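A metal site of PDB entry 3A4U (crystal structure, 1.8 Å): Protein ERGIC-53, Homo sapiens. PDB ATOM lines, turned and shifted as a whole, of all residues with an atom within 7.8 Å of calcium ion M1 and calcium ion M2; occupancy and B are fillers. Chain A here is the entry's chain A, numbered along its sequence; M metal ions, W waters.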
ATOM      1  N   GLY A  89      20.851  -8.972  -1.054  1.00  0.00           N
ATOM      2  CA  GLY A  89      19.837 -10.003  -0.808  1.00  0.00           C
ATOM      3  C   GLY A  89      18.953  -9.635   0.366  1.00  0.00           C
ATOM      4  O   GLY A  89      19.133  -8.580   0.972  1.00  0.00           O
ATOM      5  N   ALA A  90      18.007 -10.519   0.677  1.00  0.00           N
ATOM      6  CA  ALA A  90      17.083 -10.337   1.797  1.00  0.00           C
ATOM      7  C   ALA A  90      16.444 -11.678   2.170  1.00  0.00           C
ATOM      8  O   ALA A  90      16.413 -12.592   1.340  1.00  0.00           O
ATOM      9  CB  ALA A  90      15.995  -9.311   1.451  1.00  0.00           C
ATOM     10  N   ASP A  91      15.950 -11.812   3.399  1.00  0.00           N
ATOM     11  CA  ASP A  91      16.089 -10.814   4.454  1.00  0.00           C
ATOM     12  C   ASP A  91      17.190 -11.167   5.436  1.00  0.00           C
ATOM     13  O   ASP A  91      17.836 -10.285   6.008  1.00  0.00           O
ATOM     14  CB  ASP A  91      14.779 -10.665   5.216  1.00  0.00           C
ATOM     15  CG  ASP A  91      13.961  -9.522   4.698  1.00  0.00           C
ATOM     16  OD1 ASP A  91      12.973  -9.782   3.984  1.00  0.00           O
ATOM     17  OD2 ASP A  91      14.327  -8.344   4.987  1.00  0.00           O
ATOM     18  N   GLY A  92      17.377 -12.465   5.642  1.00  0.00           N
ATOM     19  CA  GLY A  92      18.426 -12.951   6.509  1.00  0.00           C
ATOM     20  C   GLY A  92      18.016 -14.176   7.297  1.00  0.00           C
ATOM     21  O   GLY A  92      16.907 -14.700   7.134  1.00  0.00           O
ATOM     22  N   PHE A 108      12.563 -12.516  11.039  1.00  0.00           N
ATOM     23  CA  PHE A 108      13.328 -13.475  10.242  1.00  0.00           C
ATOM     24  C   PHE A 108      12.646 -14.845  10.221  1.00  0.00           C
ATOM     25  O   PHE A 108      13.285 -15.884  10.383  1.00  0.00           O
ATOM     26  CB  PHE A 108      14.791 -13.548  10.734  1.00  0.00           C
ATOM     27  CG  PHE A 108      15.534 -12.243  10.571  1.00  0.00           C
ATOM     28  CD1 PHE A 108      16.100 -11.894   9.341  1.00  0.00           C
ATOM     29  CD2 PHE A 108      15.651 -11.364  11.646  1.00  0.00           C
ATOM     30  CE1 PHE A 108      16.761 -10.673   9.182  1.00  0.00           C
ATOM     31  CE2 PHE A 108      16.321 -10.138  11.495  1.00  0.00           C
ATOM     32  CZ  PHE A 108      16.874  -9.799  10.264  1.00  0.00           C
ATOM     33  N   PHE A 121      21.417 -12.574  11.335  1.00  0.00           N
ATOM     34  CA  PHE A 121      22.281 -12.384  10.177  1.00  0.00           C
ATOM     35  C   PHE A 121      21.455 -11.620   9.159  1.00  0.00           C
ATOM     36  O   PHE A 121      20.717 -12.186   8.355  1.00  0.00           O
ATOM     37  CB  PHE A 121      22.773 -13.752   9.663  1.00  0.00           C
ATOM     38  CG  PHE A 121      23.616 -14.471  10.671  1.00  0.00           C
ATOM     39  CD1 PHE A 121      24.996 -14.541  10.504  1.00  0.00           C
ATOM     40  CD2 PHE A 121      23.045 -15.020  11.811  1.00  0.00           C
ATOM     41  CE1 PHE A 121      25.786 -15.178  11.441  1.00  0.00           C
ATOM     42  CE2 PHE A 121      23.828 -15.661  12.769  1.00  0.00           C
ATOM     43  CZ  PHE A 121      25.210 -15.740  12.583  1.00  0.00           C
ATOM     44  N   ASP A 122      21.567 -10.301   9.247  1.00  0.00           N
ATOM     45  CA  ASP A 122      20.660  -9.400   8.566  1.00  0.00           C
ATOM     46  C   ASP A 122      21.284  -8.888   7.273  1.00  0.00           C
ATOM     47  O   ASP A 122      22.148  -8.004   7.288  1.00  0.00           O
ATOM     48  CB  ASP A 122      20.323  -8.229   9.502  1.00  0.00           C
ATOM     49  CG  ASP A 122      19.278  -7.295   8.916  1.00  0.00           C
ATOM     50  OD1 ASP A 122      19.026  -7.357   7.694  1.00  0.00           O
ATOM     51  OD2 ASP A 122      18.700  -6.494   9.693  1.00  0.00           O
ATOM     52  N   SER A 123      20.801  -9.417   6.146  1.00  0.00           N
ATOM     53  CA  SER A 123      21.367  -9.097   4.826  1.00  0.00           C
ATOM     54  C   SER A 123      20.922  -7.755   4.288  1.00  0.00           C
ATOM     55  O   SER A 123      21.645  -7.145   3.483  1.00  0.00           O
ATOM     56  CB  SER A 123      20.941 -10.157   3.802  1.00  0.00           C
ATOM     57  OG  SER A 123      21.321 -11.447   4.228  1.00  0.00           O
ATOM     58  N   PHE A 124      19.745  -7.312   4.692  1.00  0.00           N
ATOM     59  CA  PHE A 124      19.119  -6.163   4.040  1.00  0.00           C
ATOM     60  C   PHE A 124      19.080  -4.912   4.923  1.00  0.00           C
ATOM     61  O   PHE A 124      18.586  -4.918   6.047  1.00  0.00           O
ATOM     62  CB  PHE A 124      17.721  -6.520   3.530  1.00  0.00           C
ATOM     63  CG  PHE A 124      17.100  -5.454   2.680  1.00  0.00           C
ATOM     64  CD1 PHE A 124      17.435  -5.326   1.331  1.00  0.00           C
ATOM     65  CD2 PHE A 124      16.182  -4.557   3.235  1.00  0.00           C
ATOM     66  CE1 PHE A 124      16.853  -4.330   0.541  1.00  0.00           C
ATOM     67  CE2 PHE A 124      15.611  -3.557   2.453  1.00  0.00           C
ATOM     68  CZ  PHE A 124      15.941  -3.442   1.105  1.00  0.00           C
ATOM     69  N   ASP A 125      19.634  -3.848   4.362  1.00  0.00           N
ATOM     70  CA  ASP A 125      19.825  -2.558   5.032  1.00  0.00           C
ATOM     71  C   ASP A 125      18.513  -1.751   5.032  1.00  0.00           C
ATOM     72  O   ASP A 125      18.310  -0.877   4.193  1.00  0.00           O
ATOM     73  CB  ASP A 125      20.943  -1.835   4.273  1.00  0.00           C
ATOM     74  CG  ASP A 125      21.369  -0.511   4.907  1.00  0.00           C
ATOM     75  OD1 ASP A 125      21.207  -0.304   6.125  1.00  0.00           O
ATOM     76  OD2 ASP A 125      21.880   0.319   4.131  1.00  0.00           O
ATOM     77  N   ASN A 126      17.623  -2.060   5.977  1.00  0.00           N
ATOM     78  CA  ASN A 126      16.308  -1.412   6.041  1.00  0.00           C
ATOM     79  C   ASN A 126      16.338   0.074   6.369  1.00  0.00           C
ATOM     80  O   ASN A 126      15.403   0.804   6.002  1.00  0.00           O
ATOM     81  CB  ASN A 126      15.382  -2.134   7.014  1.00  0.00           C
ATOM     82  CG  ASN A 126      14.931  -3.465   6.485  1.00  0.00           C
ATOM     83  OD1 ASN A 126      15.550  -4.489   6.757  1.00  0.00           O
ATOM     84  ND2 ASN A 126      13.858  -3.454   5.685  1.00  0.00           N
ATOM     85  N   ASP A 127      17.378   0.511   7.068  1.00  0.00           N
ATOM     86  CA  ASP A 127      17.510   1.920   7.452  1.00  0.00           C
ATOM     87  C   ASP A 127      18.444   2.734   6.540  1.00  0.00           C
ATOM     88  O   ASP A 127      18.621   3.935   6.743  1.00  0.00           O
ATOM     89  CB  ASP A 127      17.876   2.073   8.934  1.00  0.00           C
ATOM     90  CG  ASP A 127      19.164   1.348   9.324  1.00  0.00           C
ATOM     91  OD1 ASP A 127      19.821   0.722   8.450  1.00  0.00           O
ATOM     92  OD2 ASP A 127      19.528   1.405  10.515  1.00  0.00           O
ATOM     93  N   GLY A 128      19.022   2.074   5.534  1.00  0.00           N
ATOM     94  CA  GLY A 128      19.899   2.746   4.566  1.00  0.00           C
ATOM     95  C   GLY A 128      21.171   3.327   5.163  1.00  0.00           C
ATOM     96  O   GLY A 128      21.660   4.369   4.717  1.00  0.00           O
ATOM     97  N   LYS A 129      21.708   2.664   6.176  1.00  0.00           N
ATOM     98  CA  LYS A 129      22.900   3.138   6.881  1.00  0.00           C
ATOM     99  C   LYS A 129      24.198   2.522   6.347  1.00  0.00           C
ATOM    100  O   LYS A 129      25.261   2.702   6.939  1.00  0.00           O
ATOM    101  CB  LYS A 129      22.767   2.912   8.387  1.00  0.00           C
ATOM    102  CG  LYS A 129      21.734   3.807   9.074  1.00  0.00           C
ATOM    103  CD  LYS A 129      22.107   5.282   8.948  1.00  0.00           C
ATOM    104  CE  LYS A 129      20.987   6.186   9.452  1.00  0.00           C
ATOM    105  NZ  LYS A 129      21.253   7.606   9.084  1.00  0.00           N
ATOM    106  N   LYS A 130      24.078   1.798   5.229  1.00  0.00           N
ATOM    107  CA  LYS A 130      25.227   1.228   4.511  1.00  0.00           C
ATOM    108  C   LYS A 130      26.091   0.344   5.414  1.00  0.00           C
ATOM    109  O   LYS A 130      27.325   0.331   5.317  1.00  0.00           O
ATOM    110  CB  LYS A 130      26.056   2.355   3.873  1.00  0.00           C
ATOM    111  CG  LYS A 130      25.361   3.087   2.744  1.00  0.00           C
ATOM    112  CD  LYS A 130      26.197   4.285   2.286  1.00  0.00           C
ATOM    113  CE  LYS A 130      25.867   4.695   0.864  1.00  0.00           C
ATOM    114  NZ  LYS A 130      26.593   3.861  -0.152  1.00  0.00           N
ATOM    115  N   ASN A 131      25.417  -0.391   6.294  1.00  0.00           N
ATOM    116  CA  ASN A 131      26.088  -1.215   7.287  1.00  0.00           C
ATOM    117  C   ASN A 131      25.509  -2.624   7.326  1.00  0.00           C
ATOM    118  O   ASN A 131      25.298  -3.200   8.401  1.00  0.00           O
ATOM    119  CB  ASN A 131      26.017  -0.562   8.678  1.00  0.00           C
ATOM    120  CG  ASN A 131      24.581  -0.309   9.136  1.00  0.00           C
ATOM    121  OD1 ASN A 131      23.641  -0.314   8.346  1.00  0.00           O
ATOM    122  ND2 ASN A 131      24.415  -0.064  10.435  1.00  0.00           N
ATOM    123  N   ASN A 132      25.232  -3.163   6.127  1.00  0.00           N
ATOM    124  CA  ASN A 132      24.794  -4.547   5.955  1.00  0.00           C
ATOM    125  C   ASN A 132      25.584  -5.223   4.835  1.00  0.00           C
ATOM    126  O   ASN A 132      26.144  -4.529   3.977  1.00  0.00           O
ATOM    127  CB  ASN A 132      23.302  -4.618   5.622  1.00  0.00           C
ATOM    128  CG  ASN A 132      22.436  -4.103   6.743  1.00  0.00           C
ATOM    129  OD1 ASN A 132      22.378  -2.900   6.985  1.00  0.00           O
ATOM    130  ND2 ASN A 132      21.746  -5.004   7.433  1.00  0.00           N
ATOM    131  N   PRO A 133      25.645  -6.574   4.846  1.00  0.00           N
ATOM    132  CA  PRO A 133      25.111  -7.475   5.866  1.00  0.00           C
ATOM    133  C   PRO A 133      25.756  -7.293   7.247  1.00  0.00           C
ATOM    134  O   PRO A 133      26.942  -6.966   7.349  1.00  0.00           O
ATOM    135  CB  PRO A 133      25.423  -8.866   5.302  1.00  0.00           C
ATOM    136  CG  PRO A 133      25.511  -8.652   3.834  1.00  0.00           C
ATOM    137  CD  PRO A 133      26.222  -7.340   3.730  1.00  0.00           C
ATOM    138  N   ALA A 134      24.951  -7.482   8.285  1.00  0.00           N
ATOM    139  CA  ALA A 134      25.390  -7.318   9.648  1.00  0.00           C
ATOM    140  C   ALA A 134      24.948  -8.506  10.491  1.00  0.00           C
ATOM    141  O   ALA A 134      24.003  -9.214  10.127  1.00  0.00           O
ATOM    142  CB  ALA A 134      24.852  -6.012  10.228  1.00  0.00           C
ATOM    143  N   VAL A 136      23.695  -9.176  14.296  1.00  0.00           N
ATOM    144  CA  VAL A 136      23.134  -8.337  15.353  1.00  0.00           C
ATOM    145  C   VAL A 136      22.577  -9.217  16.461  1.00  0.00           C
ATOM    146  O   VAL A 136      21.745 -10.092  16.211  1.00  0.00           O
ATOM    147  CB  VAL A 136      22.015  -7.413  14.792  1.00  0.00           C
ATOM    148  CG1 VAL A 136      21.550  -6.429  15.832  1.00  0.00           C
ATOM    149  CG2 VAL A 136      22.512  -6.643  13.544  1.00  0.00           C
ATOM    150  N   TYR A 146      10.758  -6.401  17.820  1.00  0.00           N
ATOM    151  CA  TYR A 146      11.939  -6.196  16.961  1.00  0.00           C
ATOM    152  C   TYR A 146      11.737  -4.999  16.021  1.00  0.00           C
ATOM    153  O   TYR A 146      10.717  -4.886  15.338  1.00  0.00           O
ATOM    154  CB  TYR A 146      12.242  -7.472  16.170  1.00  0.00           C
ATOM    155  CG  TYR A 146      13.286  -7.295  15.103  1.00  0.00           C
ATOM    156  CD1 TYR A 146      14.594  -6.942  15.432  1.00  0.00           C
ATOM    157  CD2 TYR A 146      12.971  -7.501  13.752  1.00  0.00           C
ATOM    158  CE1 TYR A 146      15.573  -6.780  14.442  1.00  0.00           C
ATOM    159  CE2 TYR A 146      13.937  -7.342  12.768  1.00  0.00           C
ATOM    160  CZ  TYR A 146      15.224  -6.981  13.106  1.00  0.00           C
ATOM    161  OH  TYR A 146      16.168  -6.822  12.125  1.00  0.00           O
ATOM    162  N   ASP A 147      12.725  -4.102  15.983  1.00  0.00           N
ATOM    163  CA  ASP A 147      12.662  -2.901  15.153  1.00  0.00           C
ATOM    164  C   ASP A 147      13.216  -3.236  13.766  1.00  0.00           C
ATOM    165  O   ASP A 147      14.373  -2.958  13.479  1.00  0.00           O
ATOM    166  CB  ASP A 147      13.435  -1.750  15.805  1.00  0.00           C
ATOM    167  CG  ASP A 147      13.264  -0.421  15.076  1.00  0.00           C
ATOM    168  OD1 ASP A 147      12.635  -0.362  13.998  1.00  0.00           O
ATOM    169  OD2 ASP A 147      13.783   0.591  15.594  1.00  0.00           O
ATOM    170  N   HIS A 148      12.368  -3.833  12.926  1.00  0.00           N
ATOM    171  CA  HIS A 148      12.779  -4.301  11.597  1.00  0.00           C
ATOM    172  C   HIS A 148      13.231  -3.142  10.709  1.00  0.00           C
ATOM    173  O   HIS A 148      14.239  -3.255  10.007  1.00  0.00           O
ATOM    174  CB  HIS A 148      11.654  -5.126  10.936  1.00  0.00           C
ATOM    175  CG  HIS A 148      12.101  -5.869   9.708  1.00  0.00           C
ATOM    176  ND1 HIS A 148      12.038  -5.331   8.446  1.00  0.00           N
ATOM    177  CD2 HIS A 148      12.592  -7.127   9.563  1.00  0.00           C
ATOM    178  CE1 HIS A 148      12.480  -6.220   7.562  1.00  0.00           C
ATOM    179  NE2 HIS A 148      12.830  -7.317   8.218  1.00  0.00           N
ATOM    180  N   GLN A 149      12.515  -2.029  10.770  1.00  0.00           N
ATOM    181  CA  GLN A 149      12.778  -0.862   9.921  1.00  0.00           C
ATOM    182  C   GLN A 149      14.185  -0.260  10.126  1.00  0.00           C
ATOM    183  O   GLN A 149      14.735   0.374   9.216  1.00  0.00           O
ATOM    184  CB  GLN A 149      11.696   0.209  10.114  1.00  0.00           C
ATOM    185  CG  GLN A 149      10.322  -0.197   9.563  1.00  0.00           C
ATOM    186  CD  GLN A 149       9.272   0.896   9.693  1.00  0.00           C
ATOM    187  OE1 GLN A 149       8.913   1.314  10.805  1.00  0.00           O
ATOM    188  NE2 GLN A 149       8.746   1.350   8.550  1.00  0.00           N
ATOM    189  N   ASN A 150      14.747  -0.453  11.311  1.00  0.00           N
ATOM    190  CA  ASN A 150      16.066   0.061  11.635  1.00  0.00           C
ATOM    191  C   ASN A 150      17.107  -1.038  11.889  1.00  0.00           C
ATOM    192  O   ASN A 150      18.121  -0.806  12.538  1.00  0.00           O
ATOM    193  CB  ASN A 150      15.977   1.014  12.831  1.00  0.00           C
ATOM    194  CG  ASN A 150      15.144   2.246  12.523  1.00  0.00           C
ATOM    195  OD1 ASN A 150      15.502   3.049  11.667  1.00  0.00           O
ATOM    196  ND2 ASN A 150      14.019   2.393  13.223  1.00  0.00           N
ATOM    197  N   ASP A 151      16.827  -2.241  11.365  1.00  0.00           N
ATOM    198  CA  ASP A 151      17.731  -3.388  11.528  1.00  0.00           C
ATOM    199  C   ASP A 151      18.117  -3.634  12.995  1.00  0.00           C
ATOM    200  O   ASP A 151      19.248  -4.048  13.295  1.00  0.00           O
ATOM    201  CB  ASP A 151      18.995  -3.211  10.687  1.00  0.00           C
ATOM    202  CG  ASP A 151      18.702  -3.120   9.199  1.00  0.00           C
ATOM    203  OD1 ASP A 151      17.662  -3.651   8.751  1.00  0.00           O
ATOM    204  OD2 ASP A 151      19.528  -2.539   8.474  1.00  0.00           O
ATOM    205  N   GLY A 152      17.176  -3.349  13.903  1.00  0.00           N
ATOM    206  CA  GLY A 152      17.357  -3.517  15.346  1.00  0.00           C
ATOM    207  C   GLY A 152      18.495  -2.716  15.955  1.00  0.00           C
ATOM    208  O   GLY A 152      19.006  -3.081  17.010  1.00  0.00           O
ATOM    209  N   ALA A 153      18.866  -1.608  15.313  1.00  0.00           N
ATOM    210  CA  ALA A 153      20.093  -0.881  15.650  1.00  0.00           C
ATOM    211  C   ALA A 153      20.145  -0.431  17.104  1.00  0.00           C
ATOM    212  O   ALA A 153      21.170  -0.608  17.767  1.00  0.00           O
ATOM    213  CB  ALA A 153      20.289   0.311  14.707  1.00  0.00           C
HETATM  214 CA    CA M   1      17.252  -5.710   7.799  1.00  0.00          CA
HETATM  215 CA    CA M   2      21.446  -1.184   8.383  1.00  0.00          CA
HETATM  216  O   HOH W   1      22.504  -2.926   9.796  1.00  0.00           O
HETATM  217  O   HOH W   2      16.382  -7.622   6.661  1.00  0.00           O
HETATM  218  O   HOH W   3      21.461  -0.453  10.741  1.00  0.00           O
HETATM  219  O   HOH W   4      15.487  -5.798   9.498  1.00  0.00           O
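Water W4 bridges the backbone carbonyl oxygen (O) of His 148 (2.9 Å) and the side-chain hydroxyl (OH) of Tyr 146 (2.9 Å).
Water W1 bridges the backbone carbonyl oxygen of Asn 131 (3.1 Å) and the side-chain amide nitrogen of Asn 132 (3.2 Å).
Water W3 lies within hydrogen-bond range of OD2 of Asp 127 (2.7 Å) and ND2 of Asn 131 (3.0 Å).
The backbone carbonyl oxygen (O) of Ala 134 is in hydrogen-bond range of the backbone NH (N) of Asp 122 (2.8 Å).
ND2 of Asn 132 lies close to O of Phe 124, 3.5 Å away.
OD1 of Asp 125 sits close to N of Gly 128.
N of Asp 127 sits at hydrogen-bond distance from O of Gln 149, at 3.4 Å.
The backbone NH (N) of Lys 130 is in hydrogen-bond range of the side-chain carboxylate (OD2) of Asp 125 (2.9 Å).
ND2 of Asn 132 is in hydrogen-bond range of O of Asp 122 (3.0 Å).
N of Lys 129 lies within hydrogen-bond range of OD2 of Asp 125 (3.1 Å).
Five residues have an atom within 4 Å of calcium ion M2: Asp 125, Asp 127, Asn 131, Asn 132 and Asp 151.
The side-chain carboxylate (OD2) of Asp 151 binds calcium ion M2 (2.4 Å).
OD1 of Asn 131 binds calcium ion M2 (2.4 Å).
Calcium ion M2 is bound by OD1 of Asn 132.
OD1 of Asp 125 binds calcium ion M2, at 2.4 Å.
Water W3 binds calcium ion M2 (2.5 Å).
Water W1 binds calcium ion M2.
Calcium ion M2 is bound by OD1 of Asp 127 (2.5 Å).
OD1 of Asp 151 binds calcium ion M1 (2.3 Å).
The side-chain amide oxygen (OD1) of Asn 126 binds calcium ion M1 (2.3 Å).
Calcium ion M1 is bound by O of Phe 124 (2.3 Å).
Calcium ion M1 is bound by water W2, at 2.4 Å.
The side-chain carboxylate (OD1) of Asp 122 binds calcium ion M1.
Calcium ion M1 is bound by water W4, 2.5 Å away.
OD2 of Asp 122 binds calcium ion M1.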
